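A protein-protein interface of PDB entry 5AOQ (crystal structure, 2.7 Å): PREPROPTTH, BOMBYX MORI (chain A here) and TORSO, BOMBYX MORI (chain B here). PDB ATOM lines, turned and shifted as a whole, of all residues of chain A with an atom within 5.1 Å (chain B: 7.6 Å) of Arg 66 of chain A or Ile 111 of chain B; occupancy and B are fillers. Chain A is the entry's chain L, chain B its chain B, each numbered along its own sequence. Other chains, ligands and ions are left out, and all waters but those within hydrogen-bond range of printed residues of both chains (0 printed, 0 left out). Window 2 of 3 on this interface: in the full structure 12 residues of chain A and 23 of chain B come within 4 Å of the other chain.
Of the printed residues of chain B, Asn 29 of chain A touches Asn 70. Arg 66 of chain A touches one residue of chain B. Of the printed residues of chain A, Phe 98 of chain B touches Arg 84 (3.4 Å). Of chain A, only Arg 66 (3.7 Å) comes within 4 Å of Ile 111 of chain B. The nearest residue of chain B that does not touch Arg 66 of chain A is Thr 113 of chain B (4.8 Å). The nearest residue of chain A that does not touch Ile 111 of chain B is Asn 29 of chain A (4.5 Å). The nearest printed residue of chain B that does not touch Asn 29 of chain A is Thr 112 of chain B (4.5 Å).
Of the 20 printed residues of chain B, 6 touch a printed residue of chain A. Hydrophobic or aromatic side chains of chain B that line the printed part of chain A: Pro 95, Phe 98 and Ile 111. Along chain B the printed residues that touch a printed residue of chain A span positions 70 to 113. Among the printed residues, no Asp or Glu carboxylate lies within 4 Å of a Lys or Arg side-chain nitrogen of the other chain.
The backbone NH of Thr 112 of chain B lies within hydrogen-bond range of the backbone carbonyl oxygen of Asn 70 of chain B, 2.7 Å away. The backbone NH of Arg 67 of chain A lies within hydrogen-bond range of the backbone carbonyl oxygen of Arg 84 of chain A, 3.1 Å away.
O of Ile 96 of chain B is in hydrogen-bond range of NH2 of Arg 84 of chain A.
Among the printed residues, pairs that only touch across the chains: Arg 84 of chain A with Pro 95 of chain B (3.2 Å), Arg 84 of chain A with Phe 98 of chain B (3.4 Å), Arg 67 of chain A with Thr 113 of chain B (3.5 Å), Arg 67 of chain A with Pro 95 of chain B (3.7 Å), Arg 66 of chain A with Ile 111 of chain B (3.7 Å) and Asn 29 of chain A with Asn 70 of chain B (3.8 Å).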
ATOM      1  N   ASN A  29      24.608  26.999   8.610  1.00  0.00           N
ATOM      2  CA  ASN A  29      25.981  27.087   8.123  1.00  0.00           C
ATOM      3  C   ASN A  29      26.993  26.580   9.145  1.00  0.00           C
ATOM      4  O   ASN A  29      28.126  26.250   8.793  1.00  0.00           O
ATOM      5  CB  ASN A  29      26.311  28.529   7.736  1.00  0.00           C
ATOM      6  CG  ASN A  29      25.617  28.965   6.459  1.00  0.00           C
ATOM      7  OD1 ASN A  29      24.774  28.246   5.921  1.00  0.00           O
ATOM      8  ND2 ASN A  29      25.969  30.147   5.967  1.00  0.00           N
ATOM      9  N   LEU A  64      32.028  25.924  14.070  1.00  0.00           N
ATOM     10  CA  LEU A  64      32.593  25.844  12.734  1.00  0.00           C
ATOM     11  C   LEU A  64      31.596  26.325  11.680  1.00  0.00           C
ATOM     12  O   LEU A  64      30.749  25.560  11.220  1.00  0.00           O
ATOM     13  CB  LEU A  64      33.036  24.407  12.448  1.00  0.00           C
ATOM     14  CG  LEU A  64      34.133  24.194  11.403  1.00  0.00           C
ATOM     15  CD1 LEU A  64      35.424  24.905  11.793  1.00  0.00           C
ATOM     16  CD2 LEU A  64      34.381  22.708  11.222  1.00  0.00           C
ATOM     17  N   LYS A  65      31.698  27.599  11.311  1.00  0.00           N
ATOM     18  CA  LYS A  65      30.866  28.168  10.255  1.00  0.00           C
ATOM     19  C   LYS A  65      31.560  27.931   8.914  1.00  0.00           C
ATOM     20  O   LYS A  65      32.415  27.053   8.826  1.00  0.00           O
ATOM     21  CB  LYS A  65      30.616  29.654  10.514  1.00  0.00           C
ATOM     22  CG  LYS A  65      30.094  29.917  11.922  1.00  0.00           C
ATOM     23  CD  LYS A  65      29.611  31.343  12.117  1.00  0.00           C
ATOM     24  CE  LYS A  65      29.073  31.542  13.528  1.00  0.00           C
ATOM     25  NZ  LYS A  65      28.663  32.948  13.797  1.00  0.00           N
ATOM     26  N   ARG A  66      31.210  28.689   7.875  1.00  0.00           N
ATOM     27  CA  ARG A  66      31.782  28.422   6.554  1.00  0.00           C
ATOM     28  C   ARG A  66      31.975  29.653   5.663  1.00  0.00           C
ATOM     29  O   ARG A  66      31.789  30.790   6.100  1.00  0.00           O
ATOM     30  CB  ARG A  66      30.918  27.379   5.832  1.00  0.00           C
ATOM     31  CG  ARG A  66      29.447  27.720   5.719  1.00  0.00           C
ATOM     32  CD  ARG A  66      28.701  26.601   5.011  1.00  0.00           C
ATOM     33  NE  ARG A  66      29.155  26.439   3.631  1.00  0.00           N
ATOM     34  CZ  ARG A  66      29.239  25.277   2.988  1.00  0.00           C
ATOM     35  NH1 ARG A  66      28.904  24.140   3.585  1.00  0.00           N
ATOM     36  NH2 ARG A  66      29.668  25.252   1.733  1.00  0.00           N
ATOM     37  N   ARG A  67      32.359  29.383   4.415  1.00  0.00           N
ATOM     38  CA  ARG A  67      32.870  30.367   3.456  1.00  0.00           C
ATOM     39  C   ARG A  67      32.282  31.777   3.542  1.00  0.00           C
ATOM     40  O   ARG A  67      31.071  31.975   3.431  1.00  0.00           O
ATOM     41  CB  ARG A  67      32.662  29.824   2.036  1.00  0.00           C
ATOM     42  CG  ARG A  67      33.084  30.763   0.911  1.00  0.00           C
ATOM     43  CD  ARG A  67      34.518  31.242   1.069  1.00  0.00           C
ATOM     44  NE  ARG A  67      34.924  32.111  -0.033  1.00  0.00           N
ATOM     45  CZ  ARG A  67      35.866  33.045   0.051  1.00  0.00           C
ATOM     46  NH1 ARG A  67      36.510  33.254   1.193  1.00  0.00           N
ATOM     47  NH2 ARG A  67      36.165  33.781  -1.012  1.00  0.00           N
ATOM     48  N   GLU A  68      33.175  32.743   3.737  1.00  0.00           N
ATOM     49  CA  GLU A  68      32.845  34.163   3.713  1.00  0.00           C
ATOM     50  C   GLU A  68      33.982  34.911   3.016  1.00  0.00           C
ATOM     51  O   GLU A  68      34.945  34.292   2.567  1.00  0.00           O
ATOM     52  CB  GLU A  68      32.629  34.698   5.130  1.00  0.00           C
ATOM     53  CG  GLU A  68      31.355  34.197   5.803  1.00  0.00           C
ATOM     54  CD  GLU A  68      30.096  34.837   5.244  1.00  0.00           C
ATOM     55  OE1 GLU A  68      30.163  35.995   4.781  1.00  0.00           O
ATOM     56  OE2 GLU A  68      29.034  34.177   5.271  1.00  0.00           O
ATOM     57  N   ARG A  84      37.224  26.533   3.524  1.00  0.00           N
ATOM     58  CA  ARG A  84      35.844  26.230   3.174  1.00  0.00           C
ATOM     59  C   ARG A  84      34.980  26.352   4.427  1.00  0.00           C
ATOM     60  O   ARG A  84      33.790  26.663   4.351  1.00  0.00           O
ATOM     61  CB  ARG A  84      35.745  24.823   2.582  1.00  0.00           C
ATOM     62  CG  ARG A  84      34.636  24.629   1.563  1.00  0.00           C
ATOM     63  CD  ARG A  84      34.764  23.274   0.881  1.00  0.00           C
ATOM     64  NE  ARG A  84      33.712  23.040  -0.105  1.00  0.00           N
ATOM     65  CZ  ARG A  84      33.789  23.373  -1.391  1.00  0.00           C
ATOM     66  NH1 ARG A  84      34.873  23.967  -1.874  1.00  0.00           N
ATOM     67  NH2 ARG A  84      32.773  23.112  -2.201  1.00  0.00           N
ATOM     68  N   TRP A  85      35.602  26.100   5.577  1.00  0.00           N
ATOM     69  CA  TRP A  85      34.960  26.256   6.876  1.00  0.00           C
ATOM     70  C   TRP A  85      35.726  27.275   7.721  1.00  0.00           C
ATOM     71  O   TRP A  85      36.876  27.592   7.422  1.00  0.00           O
ATOM     72  CB  TRP A  85      34.870  24.907   7.586  1.00  0.00           C
ATOM     73  CG  TRP A  85      34.061  23.916   6.808  1.00  0.00           C
ATOM     74  CD1 TRP A  85      34.520  23.049   5.860  1.00  0.00           C
ATOM     75  CD2 TRP A  85      32.647  23.703   6.895  1.00  0.00           C
ATOM     76  NE1 TRP A  85      33.481  22.306   5.356  1.00  0.00           N
ATOM     77  CE2 TRP A  85      32.320  22.688   5.975  1.00  0.00           C
ATOM     78  CE3 TRP A  85      31.626  24.270   7.664  1.00  0.00           C
ATOM     79  CZ2 TRP A  85      31.016  22.227   5.804  1.00  0.00           C
ATOM     80  CZ3 TRP A  85      30.332  23.812   7.492  1.00  0.00           C
ATOM     81  CH2 TRP A  85      30.040  22.802   6.570  1.00  0.00           C
ATOM     82  N   VAL A  86      35.078  27.788   8.765  1.00  0.00           N
ATOM     83  CA  VAL A  86      35.641  28.859   9.582  1.00  0.00           C
ATOM     84  C   VAL A  86      35.344  28.617  11.059  1.00  0.00           C
ATOM     85  O   VAL A  86      34.196  28.391  11.436  1.00  0.00           O
ATOM     86  CB  VAL A  86      35.073  30.236   9.162  1.00  0.00           C
ATOM     87  CG1 VAL A  86      35.541  31.334  10.111  1.00  0.00           C
ATOM     88  CG2 VAL A  86      35.479  30.566   7.733  1.00  0.00           C
ATOM     89  N   SER B  68      16.010  26.662   1.608  1.00  0.00           N
ATOM     90  CA  SER B  68      16.196  27.685   2.626  1.00  0.00           C
ATOM     91  C   SER B  68      17.073  28.774   2.033  1.00  0.00           C
ATOM     92  O   SER B  68      17.780  28.539   1.053  1.00  0.00           O
ATOM     93  CB  SER B  68      16.837  27.100   3.885  1.00  0.00           C
ATOM     94  OG  SER B  68      16.260  25.848   4.216  1.00  0.00           O
ATOM     95  N   ASN B  70      19.730  29.692   2.637  1.00  0.00           N
ATOM     96  CA  ASN B  70      21.130  29.287   2.607  1.00  0.00           C
ATOM     97  C   ASN B  70      21.315  27.845   2.134  1.00  0.00           C
ATOM     98  O   ASN B  70      22.419  27.307   2.210  1.00  0.00           O
ATOM     99  CB  ASN B  70      21.760  29.462   3.990  1.00  0.00           C
ATOM    100  CG  ASN B  70      21.937  30.919   4.365  1.00  0.00           C
ATOM    101  OD1 ASN B  70      22.950  31.535   4.034  1.00  0.00           O
ATOM    102  ND2 ASN B  70      20.951  31.478   5.057  1.00  0.00           N
ATOM    103  N   SER B  71      20.250  27.215   1.641  1.00  0.00           N
ATOM    104  CA  SER B  71      20.364  25.828   1.187  1.00  0.00           C
ATOM    105  C   SER B  71      19.205  25.366   0.306  1.00  0.00           C
ATOM    106  O   SER B  71      18.168  26.018   0.220  1.00  0.00           O
ATOM    107  CB  SER B  71      20.475  24.890   2.395  1.00  0.00           C
ATOM    108  OG  SER B  71      19.273  24.877   3.146  1.00  0.00           O
ATOM    109  N   ILE B  72      19.402  24.217  -0.333  1.00  0.00           N
ATOM    110  CA  ILE B  72      18.383  23.595  -1.168  1.00  0.00           C
ATOM    111  C   ILE B  72      18.361  22.098  -0.908  1.00  0.00           C
ATOM    112  O   ILE B  72      19.411  21.462  -0.890  1.00  0.00           O
ATOM    113  CB  ILE B  72      18.642  23.837  -2.677  1.00  0.00           C
ATOM    114  CG1 ILE B  72      18.627  25.329  -3.007  1.00  0.00           C
ATOM    115  CG2 ILE B  72      17.621  23.091  -3.534  1.00  0.00           C
ATOM    116  CD1 ILE B  72      19.989  25.986  -2.930  1.00  0.00           C
ATOM    117  N   ARG B  73      17.171  21.540  -0.707  1.00  0.00           N
ATOM    118  CA  ARG B  73      17.030  20.097  -0.523  1.00  0.00           C
ATOM    119  C   ARG B  73      16.208  19.514  -1.658  1.00  0.00           C
ATOM    120  O   ARG B  73      15.065  19.916  -1.892  1.00  0.00           O
ATOM    121  CB  ARG B  73      16.393  19.770   0.827  1.00  0.00           C
ATOM    122  CG  ARG B  73      17.243  20.199   2.006  1.00  0.00           C
ATOM    123  CD  ARG B  73      16.531  19.985   3.324  1.00  0.00           C
ATOM    124  NE  ARG B  73      17.220  20.670   4.411  1.00  0.00           N
ATOM    125  CZ  ARG B  73      16.806  20.684   5.673  1.00  0.00           C
ATOM    126  NH1 ARG B  73      15.699  20.044   6.024  1.00  0.00           N
ATOM    127  NH2 ARG B  73      17.505  21.339   6.586  1.00  0.00           N
ATOM    128  N   PHE B  74      16.813  18.560  -2.358  1.00  0.00           N
ATOM    129  CA  PHE B  74      16.237  17.987  -3.565  1.00  0.00           C
ATOM    130  C   PHE B  74      16.192  16.468  -3.498  1.00  0.00           C
ATOM    131  O   PHE B  74      16.833  15.848  -2.643  1.00  0.00           O
ATOM    132  CB  PHE B  74      17.048  18.416  -4.786  1.00  0.00           C
ATOM    133  CG  PHE B  74      18.502  18.059  -4.693  1.00  0.00           C
ATOM    134  CD1 PHE B  74      18.955  16.826  -5.128  1.00  0.00           C
ATOM    135  CD2 PHE B  74      19.414  18.950  -4.154  1.00  0.00           C
ATOM    136  CE1 PHE B  74      20.289  16.490  -5.034  1.00  0.00           C
ATOM    137  CE2 PHE B  74      20.749  18.620  -4.059  1.00  0.00           C
ATOM    138  CZ  PHE B  74      21.188  17.389  -4.499  1.00  0.00           C
ATOM    139  N   LEU B  87      26.051  23.158  -7.897  1.00  0.00           N
ATOM    140  CA  LEU B  87      25.328  24.400  -8.167  1.00  0.00           C
ATOM    141  C   LEU B  87      26.201  25.346  -8.978  1.00  0.00           C
ATOM    142  O   LEU B  87      27.330  25.645  -8.588  1.00  0.00           O
ATOM    143  CB  LEU B  87      24.902  25.084  -6.865  1.00  0.00           C
ATOM    144  CG  LEU B  87      23.871  24.369  -5.992  1.00  0.00           C
ATOM    145  CD1 LEU B  87      23.618  25.175  -4.731  1.00  0.00           C
ATOM    146  CD2 LEU B  87      22.575  24.148  -6.756  1.00  0.00           C
ATOM    147  N   PRO B  95      34.056  29.066  -3.836  1.00  0.00           N
ATOM    148  CA  PRO B  95      34.037  27.614  -4.054  1.00  0.00           C
ATOM    149  C   PRO B  95      32.672  27.111  -4.515  1.00  0.00           C
ATOM    150  O   PRO B  95      31.644  27.640  -4.097  1.00  0.00           O
ATOM    151  CB  PRO B  95      34.398  27.040  -2.676  1.00  0.00           C
ATOM    152  CG  PRO B  95      34.261  28.180  -1.712  1.00  0.00           C
ATOM    153  CD  PRO B  95      34.560  29.408  -2.497  1.00  0.00           C
ATOM    154  N   ILE B  96      32.674  26.094  -5.370  1.00  0.00           N
ATOM    155  CA  ILE B  96      31.444  25.612  -5.985  1.00  0.00           C
ATOM    156  C   ILE B  96      30.695  24.695  -5.020  1.00  0.00           C
ATOM    157  O   ILE B  96      31.257  23.707  -4.547  1.00  0.00           O
ATOM    158  CB  ILE B  96      31.723  24.842  -7.294  1.00  0.00           C
ATOM    159  CG1 ILE B  96      32.623  25.659  -8.224  1.00  0.00           C
ATOM    160  CG2 ILE B  96      30.414  24.497  -7.997  1.00  0.00           C
ATOM    161  CD1 ILE B  96      33.202  24.859  -9.367  1.00  0.00           C
ATOM    162  N   PRO B  97      29.427  25.020  -4.715  1.00  0.00           N
ATOM    163  CA  PRO B  97      28.633  24.097  -3.898  1.00  0.00           C
ATOM    164  C   PRO B  97      28.430  22.757  -4.586  1.00  0.00           C
ATOM    165  O   PRO B  97      28.201  22.724  -5.793  1.00  0.00           O
ATOM    166  CB  PRO B  97      27.297  24.826  -3.731  1.00  0.00           C
ATOM    167  CG  PRO B  97      27.601  26.257  -3.975  1.00  0.00           C
ATOM    168  CD  PRO B  97      28.696  26.268  -4.993  1.00  0.00           C
ATOM    169  N   PHE B  98      28.519  21.669  -3.829  1.00  0.00           N
ATOM    170  CA  PHE B  98      28.318  20.344  -4.394  1.00  0.00           C
ATOM    171  C   PHE B  98      27.839  19.363  -3.337  1.00  0.00           C
ATOM    172  O   PHE B  98      27.937  19.627  -2.140  1.00  0.00           O
ATOM    173  CB  PHE B  98      29.612  19.824  -5.024  1.00  0.00           C
ATOM    174  CG  PHE B  98      30.605  19.305  -4.020  1.00  0.00           C
ATOM    175  CD1 PHE B  98      31.474  20.167  -3.375  1.00  0.00           C
ATOM    176  CD2 PHE B  98      30.664  17.953  -3.720  1.00  0.00           C
ATOM    177  CE1 PHE B  98      32.386  19.691  -2.450  1.00  0.00           C
ATOM    178  CE2 PHE B  98      31.572  17.472  -2.796  1.00  0.00           C
ATOM    179  CZ  PHE B  98      32.435  18.342  -2.161  1.00  0.00           C
ATOM    180  N   THR B  99      27.319  18.228  -3.790  1.00  0.00           N
ATOM    181  CA  THR B  99      26.962  17.149  -2.879  1.00  0.00           C
ATOM    182  C   THR B  99      27.015  15.801  -3.585  1.00  0.00           C
ATOM    183  O   THR B  99      26.713  15.695  -4.777  1.00  0.00           O
ATOM    184  CB  THR B  99      25.560  17.365  -2.265  1.00  0.00           C
ATOM    185  OG1 THR B  99      25.289  16.332  -1.307  1.00  0.00           O
ATOM    186  CG2 THR B  99      24.479  17.356  -3.338  1.00  0.00           C
ATOM    187  N   GLU B 109      21.190  17.495  -0.431  1.00  0.00           N
ATOM    188  CA  GLU B 109      21.172  18.914  -0.100  1.00  0.00           C
ATOM    189  C   GLU B 109      22.369  19.649  -0.698  1.00  0.00           C
ATOM    190  O   GLU B 109      23.474  19.114  -0.757  1.00  0.00           O
ATOM    191  CB  GLU B 109      21.155  19.110   1.418  1.00  0.00           C
ATOM    192  CG  GLU B 109      21.049  20.569   1.850  1.00  0.00           C
ATOM    193  CD  GLU B 109      21.076  20.744   3.355  1.00  0.00           C
ATOM    194  OE1 GLU B 109      21.543  19.822   4.058  1.00  0.00           O
ATOM    195  OE2 GLU B 109      20.627  21.806   3.836  1.00  0.00           O
ATOM    196  N   LEU B 110      22.127  20.883  -1.132  1.00  0.00           N
ATOM    197  CA  LEU B 110      23.167  21.750  -1.673  1.00  0.00           C
ATOM    198  C   LEU B 110      23.133  23.095  -0.957  1.00  0.00           C
ATOM    199  O   LEU B 110      22.073  23.709  -0.814  1.00  0.00           O
ATOM    200  CB  LEU B 110      22.993  21.938  -3.180  1.00  0.00           C
ATOM    201  CG  LEU B 110      23.482  20.771  -4.041  1.00  0.00           C
ATOM    202  CD1 LEU B 110      22.824  20.790  -5.409  1.00  0.00           C
ATOM    203  CD2 LEU B 110      24.996  20.828  -4.177  1.00  0.00           C
ATOM    204  N   ILE B 111      24.302  23.542  -0.508  1.00  0.00           N
ATOM    205  CA  ILE B 111      24.404  24.743   0.313  1.00  0.00           C
ATOM    206  C   ILE B 111      24.560  26.007  -0.525  1.00  0.00           C
ATOM    207  O   ILE B 111      25.228  26.012  -1.559  1.00  0.00           O
ATOM    208  CB  ILE B 111      25.600  24.649   1.295  1.00  0.00           C
ATOM    209  CG1 ILE B 111      25.467  23.422   2.203  1.00  0.00           C
ATOM    210  CG2 ILE B 111      25.714  25.914   2.146  1.00  0.00           C
ATOM    211  CD1 ILE B 111      26.088  22.156   1.639  1.00  0.00           C
ATOM    212  N   THR B 112      23.923  27.075  -0.055  1.00  0.00           N
ATOM    213  CA  THR B 112      24.004  28.394  -0.669  1.00  0.00           C
ATOM    214  C   THR B 112      24.675  29.333   0.329  1.00  0.00           C
ATOM    215  O   THR B 112      24.526  29.157   1.539  1.00  0.00           O
ATOM    216  CB  THR B 112      22.613  28.932  -1.059  1.00  0.00           C
ATOM    217  OG1 THR B 112      22.001  28.048  -2.005  1.00  0.00           O
ATOM    218  CG2 THR B 112      22.720  30.324  -1.666  1.00  0.00           C
ATOM    219  N   THR B 113      25.410  30.323  -0.171  1.00  0.00           N
ATOM    220  CA  THR B 113      26.085  31.285   0.697  1.00  0.00           C
ATOM    221  C   THR B 113      25.515  32.694   0.546  1.00  0.00           C
ATOM    222  O   THR B 113      25.333  33.397   1.541  1.00  0.00           O
ATOM    223  CB  THR B 113      27.599  31.325   0.412  1.00  0.00           C
ATOM    224  OG1 THR B 113      28.151  30.009   0.550  1.00  0.00           O
ATOM    225  CG2 THR B 113      28.306  32.273   1.374  1.00  0.00           C
ATOM    226  N   ALA B 114      25.235  33.100  -0.689  1.00  0.00           N
ATOM    227  CA  ALA B 114      24.716  34.442  -0.958  1.00  0.00           C
ATOM    228  C   ALA B 114      23.417  34.397  -1.752  1.00  0.00           C
ATOM    229  O   ALA B 114      23.016  33.344  -2.250  1.00  0.00           O
ATOM    230  CB  ALA B 114      25.753  35.262  -1.705  1.00  0.00           C
ATOM    231  N   TYR B 118      21.442  30.080  -9.016  1.00  0.00           N
ATOM    232  CA  TYR B 118      22.301  28.949  -9.334  1.00  0.00           C
ATOM    233  C   TYR B 118      21.549  28.006 -10.258  1.00  0.00           C
ATOM    234  O   TYR B 118      20.327  28.086 -10.368  1.00  0.00           O
ATOM    235  CB  TYR B 118      22.731  28.199  -8.071  1.00  0.00           C
ATOM    236  CG  TYR B 118      23.600  28.990  -7.117  1.00  0.00           C
ATOM    237  CD1 TYR B 118      24.981  29.009  -7.254  1.00  0.00           C
ATOM    238  CD2 TYR B 118      23.039  29.704  -6.067  1.00  0.00           C
ATOM    239  CE1 TYR B 118      25.777  29.726  -6.380  1.00  0.00           C
ATOM    240  CE2 TYR B 118      23.826  30.421  -5.189  1.00  0.00           C
ATOM    241  CZ  TYR B 118      25.195  30.429  -5.348  1.00  0.00           C
ATOM    242  OH  TYR B 118      25.983  31.141  -4.473  1.00  0.00           O
ATOM    243  N   LYS B 204      17.157  16.508  11.194  1.00  0.00           N
ATOM    244  CA  LYS B 204      16.764  17.197   9.972  1.00  0.00           C
ATOM    245  C   LYS B 204      15.809  16.308   9.185  1.00  0.00           C
ATOM    246  O   LYS B 204      16.207  15.260   8.675  1.00  0.00           O
ATOM    247  CB  LYS B 204      17.995  17.536   9.131  1.00  0.00           C
ATOM    248  CG  LYS B 204      17.703  18.331   7.867  1.00  0.00           C
ATOM    249  CD  LYS B 204      18.950  18.474   7.001  1.00  0.00           C
ATOM    250  CE  LYS B 204      20.042  19.269   7.700  1.00  0.00           C
ATOM    251  NZ  LYS B 204      21.211  19.509   6.812  1.00  0.00           N
